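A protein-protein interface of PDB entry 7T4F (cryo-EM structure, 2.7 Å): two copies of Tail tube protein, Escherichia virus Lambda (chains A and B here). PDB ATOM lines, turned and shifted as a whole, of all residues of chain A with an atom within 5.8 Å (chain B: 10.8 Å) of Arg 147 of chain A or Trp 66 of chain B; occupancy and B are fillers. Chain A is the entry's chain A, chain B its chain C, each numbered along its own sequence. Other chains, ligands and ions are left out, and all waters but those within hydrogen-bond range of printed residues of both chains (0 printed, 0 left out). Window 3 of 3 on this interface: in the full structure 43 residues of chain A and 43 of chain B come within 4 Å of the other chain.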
ATOM      1  N   TYR A  26      23.231 -22.679  14.257  1.00  0.00           N
ATOM      2  CA  TYR A  26      24.672 -22.883  14.180  1.00  0.00           C
ATOM      3  C   TYR A  26      25.112 -24.226  14.748  1.00  0.00           C
ATOM      4  O   TYR A  26      26.266 -24.618  14.545  1.00  0.00           O
ATOM      5  CB  TYR A  26      25.407 -21.761  14.920  1.00  0.00           C
ATOM      6  CG  TYR A  26      25.338 -20.405  14.250  1.00  0.00           C
ATOM      7  CD1 TYR A  26      24.771 -20.253  12.991  1.00  0.00           C
ATOM      8  CD2 TYR A  26      25.843 -19.275  14.879  1.00  0.00           C
ATOM      9  CE1 TYR A  26      24.708 -19.015  12.381  1.00  0.00           C
ATOM     10  CE2 TYR A  26      25.786 -18.034  14.275  1.00  0.00           C
ATOM     11  CZ  TYR A  26      25.217 -17.910  13.026  1.00  0.00           C
ATOM     12  OH  TYR A  26      25.158 -16.675  12.423  1.00  0.00           O
ATOM     13  N   LEU A  49      32.194  -9.446   4.238  1.00  0.00           N
ATOM     14  CA  LEU A  49      32.677  -9.090   5.565  1.00  0.00           C
ATOM     15  C   LEU A  49      33.643  -7.917   5.462  1.00  0.00           C
ATOM     16  O   LEU A  49      34.619  -7.969   4.707  1.00  0.00           O
ATOM     17  CB  LEU A  49      33.361 -10.286   6.227  1.00  0.00           C
ATOM     18  CG  LEU A  49      32.610 -11.620   6.259  1.00  0.00           C
ATOM     19  CD1 LEU A  49      33.285 -12.584   7.220  1.00  0.00           C
ATOM     20  CD2 LEU A  49      31.152 -11.422   6.639  1.00  0.00           C
ATOM     21  N   GLN A  73      35.192  -1.929  14.077  1.00  0.00           N
ATOM     22  CA  GLN A  73      34.021  -2.790  14.157  1.00  0.00           C
ATOM     23  C   GLN A  73      33.837  -3.566  12.857  1.00  0.00           C
ATOM     24  O   GLN A  73      34.246  -3.125  11.779  1.00  0.00           O
ATOM     25  CB  GLN A  73      32.773  -1.960  14.461  1.00  0.00           C
ATOM     26  CG  GLN A  73      31.646  -2.743  15.114  1.00  0.00           C
ATOM     27  CD  GLN A  73      30.599  -1.843  15.736  1.00  0.00           C
ATOM     28  OE1 GLN A  73      30.118  -0.901  15.107  1.00  0.00           O
ATOM     29  NE2 GLN A  73      30.237  -2.130  16.982  1.00  0.00           N
ATOM     30  N   LYS A  74      33.209  -4.734  12.967  1.00  0.00           N
ATOM     31  CA  LYS A  74      33.031  -5.647  11.847  1.00  0.00           C
ATOM     32  C   LYS A  74      31.567  -5.702  11.434  1.00  0.00           C
ATOM     33  O   LYS A  74      30.669  -5.628  12.278  1.00  0.00           O
ATOM     34  CB  LYS A  74      33.527  -7.050  12.204  1.00  0.00           C
ATOM     35  CG  LYS A  74      34.979  -7.306  11.836  1.00  0.00           C
ATOM     36  CD  LYS A  74      35.514  -8.559  12.511  1.00  0.00           C
ATOM     37  CE  LYS A  74      35.711  -8.341  14.001  1.00  0.00           C
ATOM     38  NZ  LYS A  74      36.433  -9.475  14.639  1.00  0.00           N
ATOM     39  N   SER A  75      31.333  -5.830  10.128  1.00  0.00           N
ATOM     40  CA  SER A  75      29.994  -5.929   9.570  1.00  0.00           C
ATOM     41  C   SER A  75      29.936  -7.096   8.594  1.00  0.00           C
ATOM     42  O   SER A  75      30.933  -7.439   7.953  1.00  0.00           O
ATOM     43  CB  SER A  75      29.582  -4.633   8.860  1.00  0.00           C
ATOM     44  OG  SER A  75      28.336  -4.785   8.203  1.00  0.00           O
ATOM     45  N   ALA A  76      28.756  -7.706   8.488  1.00  0.00           N
ATOM     46  CA  ALA A  76      28.570  -8.904   7.682  1.00  0.00           C
ATOM     47  C   ALA A  76      28.025  -8.619   6.288  1.00  0.00           C
ATOM     48  O   ALA A  76      27.849  -9.559   5.506  1.00  0.00           O
ATOM     49  CB  ALA A  76      27.645  -9.886   8.407  1.00  0.00           C
ATOM     50  N   VAL A 118      26.165 -19.949   7.092  1.00  0.00           N
ATOM     51  CA  VAL A 118      24.954 -19.608   7.827  1.00  0.00           C
ATOM     52  C   VAL A 118      25.013 -18.138   8.214  1.00  0.00           C
ATOM     53  O   VAL A 118      26.009 -17.681   8.784  1.00  0.00           O
ATOM     54  CB  VAL A 118      24.776 -20.492   9.076  1.00  0.00           C
ATOM     55  CG1 VAL A 118      23.311 -20.541   9.484  1.00  0.00           C
ATOM     56  CG2 VAL A 118      25.314 -21.890   8.822  1.00  0.00           C
ATOM     57  N   ARG A 120      22.531 -14.719   9.847  1.00  0.00           N
ATOM     58  CA  ARG A 120      21.339 -14.250  10.540  1.00  0.00           C
ATOM     59  C   ARG A 120      21.077 -12.810  10.125  1.00  0.00           C
ATOM     60  O   ARG A 120      21.976 -11.966  10.210  1.00  0.00           O
ATOM     61  CB  ARG A 120      21.507 -14.339  12.058  1.00  0.00           C
ATOM     62  CG  ARG A 120      20.537 -15.286  12.743  1.00  0.00           C
ATOM     63  CD  ARG A 120      20.638 -15.174  14.256  1.00  0.00           C
ATOM     64  NE  ARG A 120      21.861 -15.774  14.776  1.00  0.00           N
ATOM     65  CZ  ARG A 120      21.901 -16.878  15.510  1.00  0.00           C
ATOM     66  NH1 ARG A 120      20.798 -17.537  15.826  1.00  0.00           N
ATOM     67  NH2 ARG A 120      23.075 -17.331  15.939  1.00  0.00           N
ATOM     68  N   VAL A 145      23.037  -9.671  10.638  1.00  0.00           N
ATOM     69  CA  VAL A 145      23.231  -9.171  11.993  1.00  0.00           C
ATOM     70  C   VAL A 145      24.141 -10.136  12.741  1.00  0.00           C
ATOM     71  O   VAL A 145      23.934 -11.354  12.696  1.00  0.00           O
ATOM     72  CB  VAL A 145      21.891  -9.003  12.732  1.00  0.00           C
ATOM     73  CG1 VAL A 145      22.122  -8.566  14.170  1.00  0.00           C
ATOM     74  CG2 VAL A 145      21.003  -8.007  12.004  1.00  0.00           C
ATOM     75  N   GLY A 146      25.144  -9.591  13.425  1.00  0.00           N
ATOM     76  CA  GLY A 146      26.007 -10.395  14.267  1.00  0.00           C
ATOM     77  C   GLY A 146      27.084 -11.137  13.495  1.00  0.00           C
ATOM     78  O   GLY A 146      27.403 -10.834  12.341  1.00  0.00           O
ATOM     79  N   ARG A 147      27.657 -12.138  14.168  1.00  0.00           N
ATOM     80  CA  ARG A 147      28.760 -12.944  13.656  1.00  0.00           C
ATOM     81  C   ARG A 147      28.230 -14.084  12.795  1.00  0.00           C
ATOM     82  O   ARG A 147      27.399 -14.870  13.264  1.00  0.00           O
ATOM     83  CB  ARG A 147      29.588 -13.511  14.800  1.00  0.00           C
ATOM     84  CG  ARG A 147      30.900 -14.143  14.369  1.00  0.00           C
ATOM     85  CD  ARG A 147      31.574 -14.854  15.530  1.00  0.00           C
ATOM     86  NE  ARG A 147      32.925 -15.290  15.194  1.00  0.00           N
ATOM     87  CZ  ARG A 147      33.225 -16.474  14.679  1.00  0.00           C
ATOM     88  NH1 ARG A 147      32.289 -17.375  14.426  1.00  0.00           N
ATOM     89  NH2 ARG A 147      34.496 -16.762  14.412  1.00  0.00           N
ATOM     90  N   PRO A 148      28.677 -14.208  11.550  1.00  0.00           N
ATOM     91  CA  PRO A 148      28.277 -15.348  10.723  1.00  0.00           C
ATOM     92  C   PRO A 148      29.052 -16.604  11.101  1.00  0.00           C
ATOM     93  O   PRO A 148      29.960 -16.589  11.934  1.00  0.00           O
ATOM     94  CB  PRO A 148      28.625 -14.886   9.306  1.00  0.00           C
ATOM     95  CG  PRO A 148      29.780 -13.970   9.508  1.00  0.00           C
ATOM     96  CD  PRO A 148      29.490 -13.239  10.794  1.00  0.00           C
ATOM     97  N   SER A 149      28.672 -17.710  10.465  1.00  0.00           N
ATOM     98  CA  SER A 149      29.298 -19.015  10.676  1.00  0.00           C
ATOM     99  C   SER A 149      29.814 -19.510   9.328  1.00  0.00           C
ATOM    100  O   SER A 149      29.105 -20.191   8.585  1.00  0.00           O
ATOM    101  CB  SER A 149      28.308 -20.002  11.305  1.00  0.00           C
ATOM    102  OG  SER A 149      28.975 -21.150  11.798  1.00  0.00           O
ATOM    103  N   ASP A 153      35.008 -22.431   9.735  1.00  0.00           N
ATOM    104  CA  ASP A 153      34.824 -22.770  11.142  1.00  0.00           C
ATOM    105  C   ASP A 153      34.635 -24.270  11.324  1.00  0.00           C
ATOM    106  O   ASP A 153      35.034 -24.835  12.349  1.00  0.00           O
ATOM    107  CB  ASP A 153      33.631 -22.005  11.715  1.00  0.00           C
ATOM    108  CG  ASP A 153      33.834 -20.504  11.688  1.00  0.00           C
ATOM    109  OD1 ASP A 153      34.703 -20.033  10.923  1.00  0.00           O
ATOM    110  OD2 ASP A 153      33.125 -19.792  12.430  1.00  0.00           O
ATOM    111  N   ASP B  55      19.555   1.278  14.820  1.00  0.00           N
ATOM    112  CA  ASP B  55      20.714   0.858  15.598  1.00  0.00           C
ATOM    113  C   ASP B  55      20.266   0.300  16.944  1.00  0.00           C
ATOM    114  O   ASP B  55      19.578   0.982  17.711  1.00  0.00           O
ATOM    115  CB  ASP B  55      21.669   2.033  15.794  1.00  0.00           C
ATOM    116  CG  ASP B  55      23.077   1.590  16.136  1.00  0.00           C
ATOM    117  OD1 ASP B  55      23.307   0.368  16.254  1.00  0.00           O
ATOM    118  OD2 ASP B  55      23.957   2.463  16.286  1.00  0.00           O
ATOM    119  N   ASP B  56      20.658  -0.941  17.231  1.00  0.00           N
ATOM    120  CA  ASP B  56      20.319  -1.606  18.483  1.00  0.00           C
ATOM    121  C   ASP B  56      21.495  -1.667  19.448  1.00  0.00           C
ATOM    122  O   ASP B  56      21.422  -2.379  20.456  1.00  0.00           O
ATOM    123  CB  ASP B  56      19.798  -3.018  18.206  1.00  0.00           C
ATOM    124  CG  ASP B  56      18.325  -3.036  17.851  1.00  0.00           C
ATOM    125  OD1 ASP B  56      17.807  -4.123  17.516  1.00  0.00           O
ATOM    126  OD2 ASP B  56      17.685  -1.966  17.906  1.00  0.00           O
ATOM    127  N   SER B  57      22.575  -0.944  19.166  1.00  0.00           N
ATOM    128  CA  SER B  57      23.766  -1.014  20.001  1.00  0.00           C
ATOM    129  C   SER B  57      23.542  -0.315  21.337  1.00  0.00           C
ATOM    130  O   SER B  57      22.816   0.679  21.426  1.00  0.00           O
ATOM    131  CB  SER B  57      24.957  -0.387  19.278  1.00  0.00           C
ATOM    132  OG  SER B  57      24.740   0.993  19.041  1.00  0.00           O
ATOM    133  N   TYR B  58      24.172  -0.848  22.381  1.00  0.00           N
ATOM    134  CA  TYR B  58      24.152  -0.257  23.709  1.00  0.00           C
ATOM    135  C   TYR B  58      25.572  -0.198  24.252  1.00  0.00           C
ATOM    136  O   TYR B  58      26.454  -0.941  23.813  1.00  0.00           O
ATOM    137  CB  TYR B  58      23.259  -1.050  24.677  1.00  0.00           C
ATOM    138  CG  TYR B  58      21.777  -0.803  24.500  1.00  0.00           C
ATOM    139  CD1 TYR B  58      21.169   0.313  25.059  1.00  0.00           C
ATOM    140  CD2 TYR B  58      20.986  -1.690  23.783  1.00  0.00           C
ATOM    141  CE1 TYR B  58      19.816   0.542  24.904  1.00  0.00           C
ATOM    142  CE2 TYR B  58      19.632  -1.470  23.622  1.00  0.00           C
ATOM    143  CZ  TYR B  58      19.052  -0.352  24.185  1.00  0.00           C
ATOM    144  OH  TYR B  58      17.704  -0.128  24.029  1.00  0.00           O
ATOM    145  N   ASP B  61      26.692  -3.624  26.389  1.00  0.00           N
ATOM    146  CA  ASP B  61      26.865  -4.952  25.809  1.00  0.00           C
ATOM    147  C   ASP B  61      28.338  -5.340  25.799  1.00  0.00           C
ATOM    148  O   ASP B  61      29.203  -4.537  25.438  1.00  0.00           O
ATOM    149  CB  ASP B  61      26.297  -5.010  24.390  1.00  0.00           C
ATOM    150  CG  ASP B  61      25.072  -4.142  24.212  1.00  0.00           C
ATOM    151  OD1 ASP B  61      24.088  -4.333  24.955  1.00  0.00           O
ATOM    152  OD2 ASP B  61      25.085  -3.287  23.303  1.00  0.00           O
ATOM    153  N   GLU B  62      28.618  -6.581  26.201  1.00  0.00           N
ATOM    154  CA  GLU B  62      29.997  -7.056  26.230  1.00  0.00           C
ATOM    155  C   GLU B  62      30.553  -7.239  24.823  1.00  0.00           C
ATOM    156  O   GLU B  62      31.712  -6.897  24.559  1.00  0.00           O
ATOM    157  CB  GLU B  62      30.085  -8.364  27.019  1.00  0.00           C
ATOM    158  CG  GLU B  62      28.990  -9.369  26.693  1.00  0.00           C
ATOM    159  CD  GLU B  62      27.806  -9.271  27.636  1.00  0.00           C
ATOM    160  OE1 GLU B  62      27.813  -8.377  28.509  1.00  0.00           O
ATOM    161  OE2 GLU B  62      26.868 -10.085  27.502  1.00  0.00           O
ATOM    162  N   ASP B  63      29.747  -7.773  23.908  1.00  0.00           N
ATOM    163  CA  ASP B  63      30.181  -8.070  22.548  1.00  0.00           C
ATOM    164  C   ASP B  63      29.840  -6.886  21.649  1.00  0.00           C
ATOM    165  O   ASP B  63      28.685  -6.717  21.244  1.00  0.00           O
ATOM    166  CB  ASP B  63      29.528  -9.353  22.039  1.00  0.00           C
ATOM    167  CG  ASP B  63      29.891  -9.662  20.598  1.00  0.00           C
ATOM    168  OD1 ASP B  63      29.194  -9.167  19.686  1.00  0.00           O
ATOM    169  OD2 ASP B  63      30.874 -10.400  20.377  1.00  0.00           O
ATOM    170  N   ALA B  64      30.847  -6.069  21.338  1.00  0.00           N
ATOM    171  CA  ALA B  64      30.695  -4.943  20.426  1.00  0.00           C
ATOM    172  C   ALA B  64      31.543  -5.103  19.170  1.00  0.00           C
ATOM    173  O   ALA B  64      31.741  -4.134  18.430  1.00  0.00           O
ATOM    174  CB  ALA B  64      31.038  -3.634  21.137  1.00  0.00           C
ATOM    175  N   ASP B  65      32.056  -6.311  18.919  1.00  0.00           N
ATOM    176  CA  ASP B  65      32.905  -6.530  17.753  1.00  0.00           C
ATOM    177  C   ASP B  65      32.108  -6.439  16.457  1.00  0.00           C
ATOM    178  O   ASP B  65      32.598  -5.907  15.455  1.00  0.00           O
ATOM    179  CB  ASP B  65      33.598  -7.889  17.858  1.00  0.00           C
ATOM    180  CG  ASP B  65      34.130  -8.165  19.251  1.00  0.00           C
ATOM    181  OD1 ASP B  65      34.393  -9.344  19.564  1.00  0.00           O
ATOM    182  OD2 ASP B  65      34.282  -7.202  20.031  1.00  0.00           O
ATOM    183  N   TRP B  66      30.880  -6.951  16.457  1.00  0.00           N
ATOM    184  CA  TRP B  66      30.045  -7.001  15.266  1.00  0.00           C
ATOM    185  C   TRP B  66      28.841  -6.088  15.437  1.00  0.00           C
ATOM    186  O   TRP B  66      28.255  -6.011  16.522  1.00  0.00           O
ATOM    187  CB  TRP B  66      29.578  -8.433  14.982  1.00  0.00           C
ATOM    188  CG  TRP B  66      30.699  -9.397  14.729  1.00  0.00           C
ATOM    189  CD1 TRP B  66      31.472 -10.016  15.666  1.00  0.00           C
ATOM    190  CD2 TRP B  66      31.169  -9.854  13.455  1.00  0.00           C
ATOM    191  NE1 TRP B  66      32.395 -10.828  15.056  1.00  0.00           N
ATOM    192  CE2 TRP B  66      32.231 -10.748  13.699  1.00  0.00           C
ATOM    193  CE3 TRP B  66      30.797  -9.596  12.133  1.00  0.00           C
ATOM    194  CZ2 TRP B  66      32.924 -11.383  12.671  1.00  0.00           C
ATOM    195  CZ3 TRP B  66      31.486 -10.226  11.113  1.00  0.00           C
ATOM    196  CH2 TRP B  66      32.536 -11.110  11.388  1.00  0.00           C
ATOM    197  N   THR B  67      28.478  -5.395  14.360  1.00  0.00           N
ATOM    198  CA  THR B  67      27.335  -4.493  14.399  1.00  0.00           C
ATOM    199  C   THR B  67      26.035  -5.278  14.518  1.00  0.00           C
ATOM    200  O   THR B  67      25.892  -6.369  13.960  1.00  0.00           O
ATOM    201  CB  THR B  67      27.302  -3.618  13.145  1.00  0.00           C
ATOM    202  OG1 THR B  67      27.018  -4.433  12.001  1.00  0.00           O
ATOM    203  CG2 THR B  67      28.637  -2.923  12.943  1.00  0.00           C
ATOM    204  N   ALA B  68      25.081  -4.713  15.255  1.00  0.00           N
ATOM    205  CA  ALA B  68      23.753  -5.292  15.406  1.00  0.00           C
ATOM    206  C   ALA B  68      22.716  -4.229  15.081  1.00  0.00           C
ATOM    207  O   ALA B  68      22.766  -3.123  15.626  1.00  0.00           O
ATOM    208  CB  ALA B  68      23.537  -5.832  16.822  1.00  0.00           C
ATOM    209  N   THR B  69      21.781  -4.565  14.195  1.00  0.00           N
ATOM    210  CA  THR B  69      20.755  -3.635  13.751  1.00  0.00           C
ATOM    211  C   THR B  69      19.405  -4.340  13.709  1.00  0.00           C
ATOM    212  O   THR B  69      19.299  -5.550  13.917  1.00  0.00           O
ATOM    213  CB  THR B  69      21.084  -3.046  12.371  1.00  0.00           C
ATOM    214  OG1 THR B  69      21.641  -4.067  11.535  1.00  0.00           O
ATOM    215  CG2 THR B  69      22.077  -1.903  12.500  1.00  0.00           C
ATOM    216  N   GLY B  70      18.366  -3.554  13.435  1.00  0.00           N
ATOM    217  CA  GLY B  70      17.028  -4.091  13.293  1.00  0.00           C
ATOM    218  C   GLY B  70      16.279  -3.366  12.196  1.00  0.00           C
ATOM    219  O   GLY B  70      16.725  -2.339  11.681  1.00  0.00           O
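The backbone carbonyl oxygen of Ala 64 of chain B lies within hydrogen-bond range of the side-chain amide nitrogen of Gln 73 of chain A (2.9 Å). N of Thr 67 of chain B sits at hydrogen-bond distance from O of Lys 74 of chain A, at 3.0 Å. N of Gly 146 of chain A sits at hydrogen-bond distance from O of Thr 67 of chain B (3.4 Å). N of Lys 74 of chain A is in hydrogen-bond range of O of Asp 65 of chain B (2.8 Å).
The side-chain hydroxyl of Tyr 26 of chain A sits at hydrogen-bond distance from the backbone carbonyl oxygen of Arg 147 of chain A (3.0 Å). O of Arg 120 of chain A sits at hydrogen-bond distance from N of Val 145 of chain A. The side-chain carboxylate (OD2) of Asp 153 of chain A is in salt-bridge range of the guanidinium group (NH1) of Arg 147 of chain A, at 3.2 Å. The backbone NH of Asp 56 of chain B is in hydrogen-bond range of the backbone carbonyl oxygen of Ala 68 of chain B.
Among the printed residues, pairs that only touch across the chains: Gln 73 of chain A with Asp 65 of chain B, Gln 73 of chain A with Thr 67 of chain B, Lys 74 of chain A with Trp 66 of chain B, Val 145 of chain A with Ala 68 of chain B, Val 145 of chain A with Thr 69 of chain B, Gly 146 of chain A with Trp 66 of chain B, Arg 147 of chain A with Trp 66 of chain B and Pro 148 of chain A with Trp 66 of chain B.
Lys 74 of chain A touches just these residues of chain B: Asp 65 (2.8 Å), Trp 66 (3.3 Å) and Thr 67 (3.0 Å). No residue of chain B comes within 4 Å of Ala 76 of chain A. Printed residues of chain B within 4 Å of Val 145 of chain A: Ala 68 (3.9 Å) and Thr 69 (3.5 Å). Gly 146 of chain A touches two residues of chain B. Arg 147 of chain A touches just one residue of chain B: Trp 66 (3.7 Å). Pro 148 of chain A touches just one residue of chain B: Trp 66. Of chain A, only Lys 74, Gly 146, Arg 147 and Pro 148 come within 4 Å of Trp 66 of chain B. Of the printed residues of chain A, Thr 67 of chain B touches Gln 73 (3.3 Å), Lys 74 (3.0 Å) and Gly 146 (3.4 Å). The nearest residue of chain B that does not touch Arg 147 of chain A is Thr 67 of chain B (6.0 Å). The nearest printed residue of chain A that does not touch Ala 64 of chain B is Lys 74 of chain A (5.7 Å).
Printed residues of chain B that touch a printed residue of chain A: Ala 64, Asp 65, Trp 66, Thr 67, Ala 68 and Thr 69. Hydrophobic or aromatic side chains of chain A within 4 Å of the printed part of chain B: Val 145 and Pro 148. Along chain A the printed residues that touch a printed residue of chain B span positions 73 to 148. Among the printed residues, no Asp or Glu carboxylate lies within 4 Å of a Lys or Arg side-chain nitrogen of the other chain.
No position is printed for both chains. Of the 12 pairs that touch across the chains among the printed residues, none has its exchanged pair printed and touching as well.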
